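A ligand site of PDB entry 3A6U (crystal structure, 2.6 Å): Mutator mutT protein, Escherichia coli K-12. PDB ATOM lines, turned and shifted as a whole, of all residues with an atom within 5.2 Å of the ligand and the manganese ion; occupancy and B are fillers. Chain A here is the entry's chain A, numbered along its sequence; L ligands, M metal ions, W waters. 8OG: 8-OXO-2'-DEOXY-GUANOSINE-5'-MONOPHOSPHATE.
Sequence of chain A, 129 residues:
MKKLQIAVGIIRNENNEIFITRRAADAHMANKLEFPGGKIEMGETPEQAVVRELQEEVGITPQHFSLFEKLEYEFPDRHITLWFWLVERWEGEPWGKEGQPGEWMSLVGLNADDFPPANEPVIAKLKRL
Merely in contact with the ligand: Ile 6 (3.7 Å), Val 8 (3.3 Å), Pro 36 (3.9 Å), Gly 38 (3.8 Å), Phe 75 (3.5 Å), Leu 82 (3.7 Å), Pro 116 (3.5 Å) and Ala 118 (3.7 Å). Hydrophobic or aromatic side chains that line the ligand: Ile 6, Val 8, His 28, Phe 35, Phe 75, Leu 82, Pro 116 and Ala 118.
The nearest printed residue that does not touch the manganese ion is Gly 38 (4.1 Å).
NH2 of Arg 23 is in hydrogen-bond range of O of His 28. The guanidinium group (NH1) of Arg 23 lies within salt-bridge range of the side-chain carboxylate (OE2) of Glu 34, 2.8 Å away. The guanidinium group (NE) of Arg 23 lies close to the backbone carbonyl oxygen (O) of Met 29 (3.1 Å). The guanidinium group of Arg 78 lies close to a ring nitrogen (NE2) of His 28 (3.4 Å).
The manganese ion is bound by water W3 (2.1 Å), water W7 (2.1 Å), water W4 (2.2 Å), the backbone carbonyl oxygen (O) of Gly 37 (2.2 Å), an oxygen (OP1) of the ligand (2.2 Å) and the side-chain carboxylate (OE1) of Glu 57 (2.3 Å). The manganese ion has six donor atoms within binding distance.
An oxygen (O6) of the ligand sits at hydrogen-bond distance from the backbone NH of Phe 35 (3.0 Å). O of Phe 35 sits at hydrogen-bond distance from N1 of the ligand (2.6 Å). OP3 of the ligand lies within salt-bridge range of NH2 of Arg 23 (2.7 Å). OD1 of Asn 119 lies within hydrogen-bond range of N7 of the ligand (2.8 Å). O3' of the ligand sits at hydrogen-bond distance from ND1 of His 28 (2.8 Å). The side-chain carboxylate (OE2) of Glu 34 is in hydrogen-bond range of a nitrogen (N2) of the ligand, at 3.0 Å.
Water W7 lies within hydrogen-bond range of OE2 of Glu 57 (2.8 Å), OE2 of Glu 34 (2.9 Å), N2 of the ligand (3.1 Å) and N of Gly 37 (3.5 Å). Water W1 bridges OP3 of the ligand (2.5 Å) and NH2 of Arg 23 (3.4 Å). Water W5 lies within hydrogen-bond range of OP2 of the ligand and N of Lys 39. Water W2 lies within hydrogen-bond range of the guanidinium group (NH1) of Arg 78 and an oxygen (O3') of the ligand.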
ATOM      1  N   ILE A   6     -16.674  28.151 -18.861  1.00  0.00           N
ATOM      2  CA  ILE A   6     -17.778  27.180 -18.971  1.00  0.00           C
ATOM      3  C   ILE A   6     -17.346  25.715 -19.015  1.00  0.00           C
ATOM      4  O   ILE A   6     -16.459  25.337 -19.777  1.00  0.00           O
ATOM      5  CB  ILE A   6     -18.623  27.489 -20.234  1.00  0.00           C
ATOM      6  CG1 ILE A   6     -19.051  28.959 -20.221  1.00  0.00           C
ATOM      7  CG2 ILE A   6     -19.834  26.559 -20.299  1.00  0.00           C
ATOM      8  CD1 ILE A   6     -19.851  29.361 -19.005  1.00  0.00           C
ATOM      9  N   VAL A   8     -18.652  21.807 -19.645  1.00  0.00           N
ATOM     10  CA  VAL A   8     -19.718  21.016 -20.247  1.00  0.00           C
ATOM     11  C   VAL A   8     -19.327  19.551 -20.312  1.00  0.00           C
ATOM     12  O   VAL A   8     -18.131  19.227 -20.400  1.00  0.00           O
ATOM     13  CB  VAL A   8     -20.064  21.524 -21.660  1.00  0.00           C
ATOM     14  CG1 VAL A   8     -20.456  22.993 -21.604  1.00  0.00           C
ATOM     15  CG2 VAL A   8     -18.870  21.329 -22.586  1.00  0.00           C
ATOM     16  N   ARG A  23     -31.216  24.232 -25.935  1.00  0.00           N
ATOM     17  CA  ARG A  23     -31.292  25.452 -25.141  1.00  0.00           C
ATOM     18  C   ARG A  23     -32.608  26.190 -25.316  1.00  0.00           C
ATOM     19  O   ARG A  23     -33.167  26.255 -26.416  1.00  0.00           O
ATOM     20  CB  ARG A  23     -30.113  26.365 -25.483  1.00  0.00           C
ATOM     21  CG  ARG A  23     -28.772  25.737 -25.199  1.00  0.00           C
ATOM     22  CD  ARG A  23     -27.629  26.601 -25.686  1.00  0.00           C
ATOM     23  NE  ARG A  23     -27.577  27.866 -24.962  1.00  0.00           N
ATOM     24  CZ  ARG A  23     -27.190  27.997 -23.696  1.00  0.00           C
ATOM     25  NH1 ARG A  23     -26.808  26.937 -22.998  1.00  0.00           N
ATOM     26  NH2 ARG A  23     -27.188  29.201 -23.134  1.00  0.00           N
ATOM     27  N   HIS A  28     -28.949  32.654 -24.170  1.00  0.00           N
ATOM     28  CA  HIS A  28     -27.901  32.992 -25.123  1.00  0.00           C
ATOM     29  C   HIS A  28     -27.780  31.718 -25.956  1.00  0.00           C
ATOM     30  O   HIS A  28     -27.901  30.619 -25.407  1.00  0.00           O
ATOM     31  CB  HIS A  28     -26.581  33.281 -24.382  1.00  0.00           C
ATOM     32  CG  HIS A  28     -25.419  33.546 -25.283  1.00  0.00           C
ATOM     33  ND1 HIS A  28     -24.477  32.590 -25.582  1.00  0.00           N
ATOM     34  CD2 HIS A  28     -25.054  34.662 -25.962  1.00  0.00           C
ATOM     35  CE1 HIS A  28     -23.574  33.104 -26.400  1.00  0.00           C
ATOM     36  NE2 HIS A  28     -23.895  34.359 -26.639  1.00  0.00           N
ATOM     37  N   MET A  29     -27.561  31.861 -27.248  1.00  0.00           N
ATOM     38  CA  MET A  29     -27.483  30.698 -28.126  1.00  0.00           C
ATOM     39  C   MET A  29     -28.761  29.883 -27.967  1.00  0.00           C
ATOM     40  O   MET A  29     -28.728  28.660 -27.773  1.00  0.00           O
ATOM     41  CB  MET A  29     -26.248  29.871 -27.792  1.00  0.00           C
ATOM     42  CG  MET A  29     -24.935  30.527 -28.196  1.00  0.00           C
ATOM     43  SD  MET A  29     -24.949  31.012 -29.961  1.00  0.00           S
ATOM     44  CE  MET A  29     -24.487  29.573 -30.650  1.00  0.00           C
ATOM     45  N   GLU A  34     -26.733  21.356 -27.444  1.00  0.00           N
ATOM     46  CA  GLU A  34     -25.620  21.641 -26.556  1.00  0.00           C
ATOM     47  C   GLU A  34     -25.238  20.445 -25.712  1.00  0.00           C
ATOM     48  O   GLU A  34     -25.973  19.452 -25.653  1.00  0.00           O
ATOM     49  CB  GLU A  34     -26.014  22.766 -25.588  1.00  0.00           C
ATOM     50  CG  GLU A  34     -27.191  22.355 -24.713  1.00  0.00           C
ATOM     51  CD  GLU A  34     -27.359  23.190 -23.458  1.00  0.00           C
ATOM     52  OE1 GLU A  34     -28.285  22.860 -22.683  1.00  0.00           O
ATOM     53  OE2 GLU A  34     -26.584  24.167 -23.237  1.00  0.00           O
ATOM     54  N   PHE A  35     -24.076  20.542 -25.071  1.00  0.00           N
ATOM     55  CA  PHE A  35     -23.594  19.510 -24.162  1.00  0.00           C
ATOM     56  C   PHE A  35     -24.002  20.100 -22.819  1.00  0.00           C
ATOM     57  O   PHE A  35     -23.745  21.278 -22.565  1.00  0.00           O
ATOM     58  CB  PHE A  35     -22.071  19.379 -24.208  1.00  0.00           C
ATOM     59  CG  PHE A  35     -21.531  18.929 -25.530  1.00  0.00           C
ATOM     60  CD1 PHE A  35     -21.880  17.681 -26.049  1.00  0.00           C
ATOM     61  CD2 PHE A  35     -20.650  19.734 -26.251  1.00  0.00           C
ATOM     62  CE1 PHE A  35     -21.370  17.252 -27.271  1.00  0.00           C
ATOM     63  CE2 PHE A  35     -20.132  19.314 -27.480  1.00  0.00           C
ATOM     64  CZ  PHE A  35     -20.494  18.065 -27.988  1.00  0.00           C
ATOM     65  N   PRO A  36     -24.652  19.316 -21.950  1.00  0.00           N
ATOM     66  CA  PRO A  36     -25.022  19.950 -20.676  1.00  0.00           C
ATOM     67  C   PRO A  36     -23.809  20.615 -20.005  1.00  0.00           C
ATOM     68  O   PRO A  36     -22.701  20.062 -20.013  1.00  0.00           O
ATOM     69  CB  PRO A  36     -25.576  18.777 -19.875  1.00  0.00           C
ATOM     70  CG  PRO A  36     -26.169  17.885 -20.960  1.00  0.00           C
ATOM     71  CD  PRO A  36     -25.103  17.920 -22.016  1.00  0.00           C
ATOM     72  N   GLY A  37     -24.022  21.794 -19.439  1.00  0.00           N
ATOM     73  CA  GLY A  37     -22.939  22.501 -18.778  1.00  0.00           C
ATOM     74  C   GLY A  37     -23.352  23.844 -18.216  1.00  0.00           C
ATOM     75  O   GLY A  37     -24.487  24.287 -18.372  1.00  0.00           O
ATOM     76  N   GLY A  38     -22.422  24.520 -17.566  1.00  0.00           N
ATOM     77  CA  GLY A  38     -22.721  25.807 -16.989  1.00  0.00           C
ATOM     78  C   GLY A  38     -21.480  26.511 -16.489  1.00  0.00           C
ATOM     79  O   GLY A  38     -20.374  25.964 -16.561  1.00  0.00           O
ATOM     80  N   LYS A  39     -21.672  27.716 -15.977  1.00  0.00           N
ATOM     81  CA  LYS A  39     -20.572  28.532 -15.486  1.00  0.00           C
ATOM     82  C   LYS A  39     -19.803  27.902 -14.322  1.00  0.00           C
ATOM     83  O   LYS A  39     -20.409  27.393 -13.375  1.00  0.00           O
ATOM     84  CB  LYS A  39     -21.113  29.892 -15.057  1.00  0.00           C
ATOM     85  CG  LYS A  39     -20.065  30.848 -14.530  1.00  0.00           C
ATOM     86  CD  LYS A  39     -20.718  32.109 -13.979  1.00  0.00           C
ATOM     87  CE  LYS A  39     -19.689  33.127 -13.499  1.00  0.00           C
ATOM     88  NZ  LYS A  39     -18.803  32.581 -12.442  1.00  0.00           N
ATOM     89  N   GLU A  53     -22.704  20.505 -12.503  1.00  0.00           N
ATOM     90  CA  GLU A  53     -23.574  20.874 -13.614  1.00  0.00           C
ATOM     91  C   GLU A  53     -24.351  19.713 -14.225  1.00  0.00           C
ATOM     92  O   GLU A  53     -25.544  19.850 -14.540  1.00  0.00           O
ATOM     93  CB  GLU A  53     -22.742  21.563 -14.713  1.00  0.00           C
ATOM     94  CG  GLU A  53     -22.333  22.998 -14.371  1.00  0.00           C
ATOM     95  CD  GLU A  53     -23.499  23.965 -14.428  1.00  0.00           C
ATOM     96  OE1 GLU A  53     -23.321  25.138 -14.052  1.00  0.00           O
ATOM     97  OE2 GLU A  53     -24.602  23.552 -14.845  1.00  0.00           O
ATOM     98  N   GLU A  57     -28.293  19.504 -14.272  1.00  0.00           N
ATOM     99  CA  GLU A  57     -29.010  19.452 -15.546  1.00  0.00           C
ATOM    100  C   GLU A  57     -29.544  18.109 -16.041  1.00  0.00           C
ATOM    101  O   GLU A  57     -30.634  18.073 -16.620  1.00  0.00           O
ATOM    102  CB  GLU A  57     -28.158  20.101 -16.643  1.00  0.00           C
ATOM    103  CG  GLU A  57     -28.007  21.597 -16.443  1.00  0.00           C
ATOM    104  CD  GLU A  57     -27.463  22.300 -17.649  1.00  0.00           C
ATOM    105  OE1 GLU A  57     -27.417  23.546 -17.624  1.00  0.00           O
ATOM    106  OE2 GLU A  57     -27.079  21.620 -18.612  1.00  0.00           O
ATOM    107  N   PHE A  75     -18.067  35.559 -28.639  1.00  0.00           N
ATOM    108  CA  PHE A  75     -19.412  35.753 -29.167  1.00  0.00           C
ATOM    109  C   PHE A  75     -19.612  37.263 -29.373  1.00  0.00           C
ATOM    110  O   PHE A  75     -18.891  38.080 -28.794  1.00  0.00           O
ATOM    111  CB  PHE A  75     -20.442  35.214 -28.168  1.00  0.00           C
ATOM    112  CG  PHE A  75     -20.568  33.729 -28.185  1.00  0.00           C
ATOM    113  CD1 PHE A  75     -21.299  33.092 -29.188  1.00  0.00           C
ATOM    114  CD2 PHE A  75     -19.960  32.950 -27.211  1.00  0.00           C
ATOM    115  CE1 PHE A  75     -21.423  31.701 -29.215  1.00  0.00           C
ATOM    116  CE2 PHE A  75     -20.074  31.559 -27.228  1.00  0.00           C
ATOM    117  CZ  PHE A  75     -20.810  30.931 -28.226  1.00  0.00           C
ATOM    118  N   ARG A  78     -20.039  38.486 -25.722  1.00  0.00           N
ATOM    119  CA  ARG A  78     -19.334  37.888 -24.595  1.00  0.00           C
ATOM    120  C   ARG A  78     -18.207  36.957 -25.032  1.00  0.00           C
ATOM    121  O   ARG A  78     -18.230  36.411 -26.130  1.00  0.00           O
ATOM    122  CB  ARG A  78     -20.325  37.141 -23.688  1.00  0.00           C
ATOM    123  CG  ARG A  78     -20.834  35.825 -24.259  1.00  0.00           C
ATOM    124  CD  ARG A  78     -22.112  35.397 -23.567  1.00  0.00           C
ATOM    125  NE  ARG A  78     -23.209  36.308 -23.886  1.00  0.00           N
ATOM    126  CZ  ARG A  78     -24.364  36.374 -23.236  1.00  0.00           C
ATOM    127  NH1 ARG A  78     -24.600  35.568 -22.198  1.00  0.00           N
ATOM    128  NH2 ARG A  78     -25.291  37.238 -23.616  1.00  0.00           N
ATOM    129  N   ILE A  80     -16.155  33.562 -23.852  1.00  0.00           N
ATOM    130  CA  ILE A  80     -16.171  32.453 -22.911  1.00  0.00           C
ATOM    131  C   ILE A  80     -15.160  31.356 -23.225  1.00  0.00           C
ATOM    132  O   ILE A  80     -14.836  31.076 -24.381  1.00  0.00           O
ATOM    133  CB  ILE A  80     -17.588  31.823 -22.781  1.00  0.00           C
ATOM    134  CG1 ILE A  80     -18.063  31.293 -24.127  1.00  0.00           C
ATOM    135  CG2 ILE A  80     -18.568  32.857 -22.254  1.00  0.00           C
ATOM    136  CD1 ILE A  80     -17.692  29.854 -24.369  1.00  0.00           C
ATOM    137  N   LEU A  82     -14.449  27.467 -22.929  1.00  0.00           N
ATOM    138  CA  LEU A  82     -15.163  26.207 -22.790  1.00  0.00           C
ATOM    139  C   LEU A  82     -14.256  25.044 -22.388  1.00  0.00           C
ATOM    140  O   LEU A  82     -13.191  24.851 -22.964  1.00  0.00           O
ATOM    141  CB  LEU A  82     -15.869  25.866 -24.105  1.00  0.00           C
ATOM    142  CG  LEU A  82     -17.100  26.714 -24.451  1.00  0.00           C
ATOM    143  CD1 LEU A  82     -17.450  26.566 -25.916  1.00  0.00           C
ATOM    144  CD2 LEU A  82     -18.259  26.267 -23.583  1.00  0.00           C
ATOM    145  N   PHE A  84     -14.422  21.212 -22.387  1.00  0.00           N
ATOM    146  CA  PHE A  84     -15.152  20.040 -22.871  1.00  0.00           C
ATOM    147  C   PHE A  84     -14.655  18.728 -22.265  1.00  0.00           C
ATOM    148  O   PHE A  84     -13.599  18.226 -22.635  1.00  0.00           O
ATOM    149  CB  PHE A  84     -15.040  19.960 -24.392  1.00  0.00           C
ATOM    150  CG  PHE A  84     -15.696  21.094 -25.126  1.00  0.00           C
ATOM    151  CD1 PHE A  84     -17.046  21.040 -25.441  1.00  0.00           C
ATOM    152  CD2 PHE A  84     -14.960  22.208 -25.526  1.00  0.00           C
ATOM    153  CE1 PHE A  84     -17.660  22.071 -26.147  1.00  0.00           C
ATOM    154  CE2 PHE A  84     -15.561  23.256 -26.225  1.00  0.00           C
ATOM    155  CZ  PHE A  84     -16.915  23.190 -26.546  1.00  0.00           C
ATOM    156  N   PHE A 115     -25.314  23.230 -33.153  1.00  0.00           N
ATOM    157  CA  PHE A 115     -24.718  23.630 -31.884  1.00  0.00           C
ATOM    158  C   PHE A 115     -24.140  25.022 -31.990  1.00  0.00           C
ATOM    159  O   PHE A 115     -24.196  25.647 -33.053  1.00  0.00           O
ATOM    160  CB  PHE A 115     -23.582  22.677 -31.486  1.00  0.00           C
ATOM    161  CG  PHE A 115     -24.019  21.259 -31.241  1.00  0.00           C
ATOM    162  CD1 PHE A 115     -24.488  20.461 -32.273  1.00  0.00           C
ATOM    163  CD2 PHE A 115     -23.957  20.712 -29.951  1.00  0.00           C
ATOM    164  CE1 PHE A 115     -24.891  19.142 -32.036  1.00  0.00           C
ATOM    165  CE2 PHE A 115     -24.364  19.397 -29.701  1.00  0.00           C
ATOM    166  CZ  PHE A 115     -24.824  18.612 -30.749  1.00  0.00           C
ATOM    167  N   PRO A 116     -23.597  25.558 -30.876  1.00  0.00           N
ATOM    168  CA  PRO A 116     -23.018  26.896 -30.975  1.00  0.00           C
ATOM    169  C   PRO A 116     -21.763  26.797 -31.822  1.00  0.00           C
ATOM    170  O   PRO A 116     -21.057  25.789 -31.784  1.00  0.00           O
ATOM    171  CB  PRO A 116     -22.739  27.243 -29.512  1.00  0.00           C
ATOM    172  CG  PRO A 116     -23.877  26.560 -28.803  1.00  0.00           C
ATOM    173  CD  PRO A 116     -23.859  25.197 -29.477  1.00  0.00           C
ATOM    174  N   ALA A 118     -18.992  27.698 -31.387  1.00  0.00           N
ATOM    175  CA  ALA A 118     -17.833  27.404 -30.547  1.00  0.00           C
ATOM    176  C   ALA A 118     -17.515  25.906 -30.505  1.00  0.00           C
ATOM    177  O   ALA A 118     -16.364  25.524 -30.352  1.00  0.00           O
ATOM    178  CB  ALA A 118     -18.068  27.931 -29.129  1.00  0.00           C
ATOM    179  N   ASN A 119     -18.537  25.065 -30.654  1.00  0.00           N
ATOM    180  CA  ASN A 119     -18.395  23.613 -30.629  1.00  0.00           C
ATOM    181  C   ASN A 119     -17.878  22.991 -31.933  1.00  0.00           C
ATOM    182  O   ASN A 119     -17.608  21.781 -31.994  1.00  0.00           O
ATOM    183  CB  ASN A 119     -19.736  22.970 -30.284  1.00  0.00           C
ATOM    184  CG  ASN A 119     -20.266  23.410 -28.934  1.00  0.00           C
ATOM    185  OD1 ASN A 119     -19.982  24.504 -28.455  1.00  0.00           O
ATOM    186  ND2 ASN A 119     -21.080  22.557 -28.316  1.00  0.00           N
HETATM  187  OP3 8OG L   1     -26.411  28.916 -20.612  1.00  0.00           O
HETATM  188  P   8OG L   1     -25.436  28.643 -19.524  1.00  0.00           P
HETATM  189  OP1 8OG L   1     -25.438  27.183 -19.321  1.00  0.00           O
HETATM  190  OP2 8OG L   1     -25.795  29.532 -18.394  1.00  0.00           O
HETATM  191  O5' 8OG L   1     -23.973  29.111 -20.056  1.00  0.00           O
HETATM  192  C5' 8OG L   1     -23.302  28.386 -21.104  1.00  0.00           C
HETATM  193  C4' 8OG L   1     -22.617  29.342 -22.102  1.00  0.00           C
HETATM  194  O4' 8OG L   1     -21.634  28.628 -22.885  1.00  0.00           O
HETATM  195  C3' 8OG L   1     -23.611  29.946 -23.096  1.00  0.00           C
HETATM  196  O3' 8OG L   1     -23.272  31.318 -23.361  1.00  0.00           O
HETATM  197  C2' 8OG L   1     -23.504  29.085 -24.318  1.00  0.00           C
HETATM  198  C1' 8OG L   1     -22.053  28.594 -24.281  1.00  0.00           C
HETATM  199  N9  8OG L   1     -21.938  27.208 -24.824  1.00  0.00           N
HETATM  200  C8  8OG L   1     -21.323  26.895 -26.003  1.00  0.00           C
HETATM  201  N7  8OG L   1     -21.298  25.667 -26.311  1.00  0.00           N
HETATM  202  C5  8OG L   1     -21.957  25.011 -25.256  1.00  0.00           C
HETATM  203  C6  8OG L   1     -22.256  23.633 -25.006  1.00  0.00           C
HETATM  204  O6  8OG L   1     -21.991  22.655 -25.688  1.00  0.00           O
HETATM  205  N1  8OG L   1     -22.946  23.470 -23.789  1.00  0.00           N
HETATM  206  C2  8OG L   1     -23.311  24.480 -22.911  1.00  0.00           C
HETATM  207  N2  8OG L   1     -23.954  24.121 -21.802  1.00  0.00           N
HETATM  208  N3  8OG L   1     -23.024  25.780 -23.143  1.00  0.00           N
HETATM  209  C4  8OG L   1     -22.353  25.987 -24.317  1.00  0.00           C
HETATM  210  O8  8OG L   1     -20.843  27.813 -26.682  1.00  0.00           O
HETATM  211 MN    MN M   1     -26.388  25.239 -18.818  1.00  0.00          MN
HETATM  212  O   HOH W   1     -28.821  28.224 -20.320  1.00  0.00           O
HETATM  213  O   HOH W   2     -23.555  33.238 -21.365  1.00  0.00           O
HETATM  214  O   HOH W   3     -26.730  25.901 -16.864  1.00  0.00           O
HETATM  215  O   HOH W   4     -28.481  25.523 -19.306  1.00  0.00           O
HETATM  216  O   HOH W   5     -24.237  28.611 -16.345  1.00  0.00           O
HETATM  217  O   HOH W   6     -26.113  31.821 -20.321  1.00  0.00           O
HETATM  218  O   HOH W   7     -26.712  23.807 -20.350  1.00  0.00           O
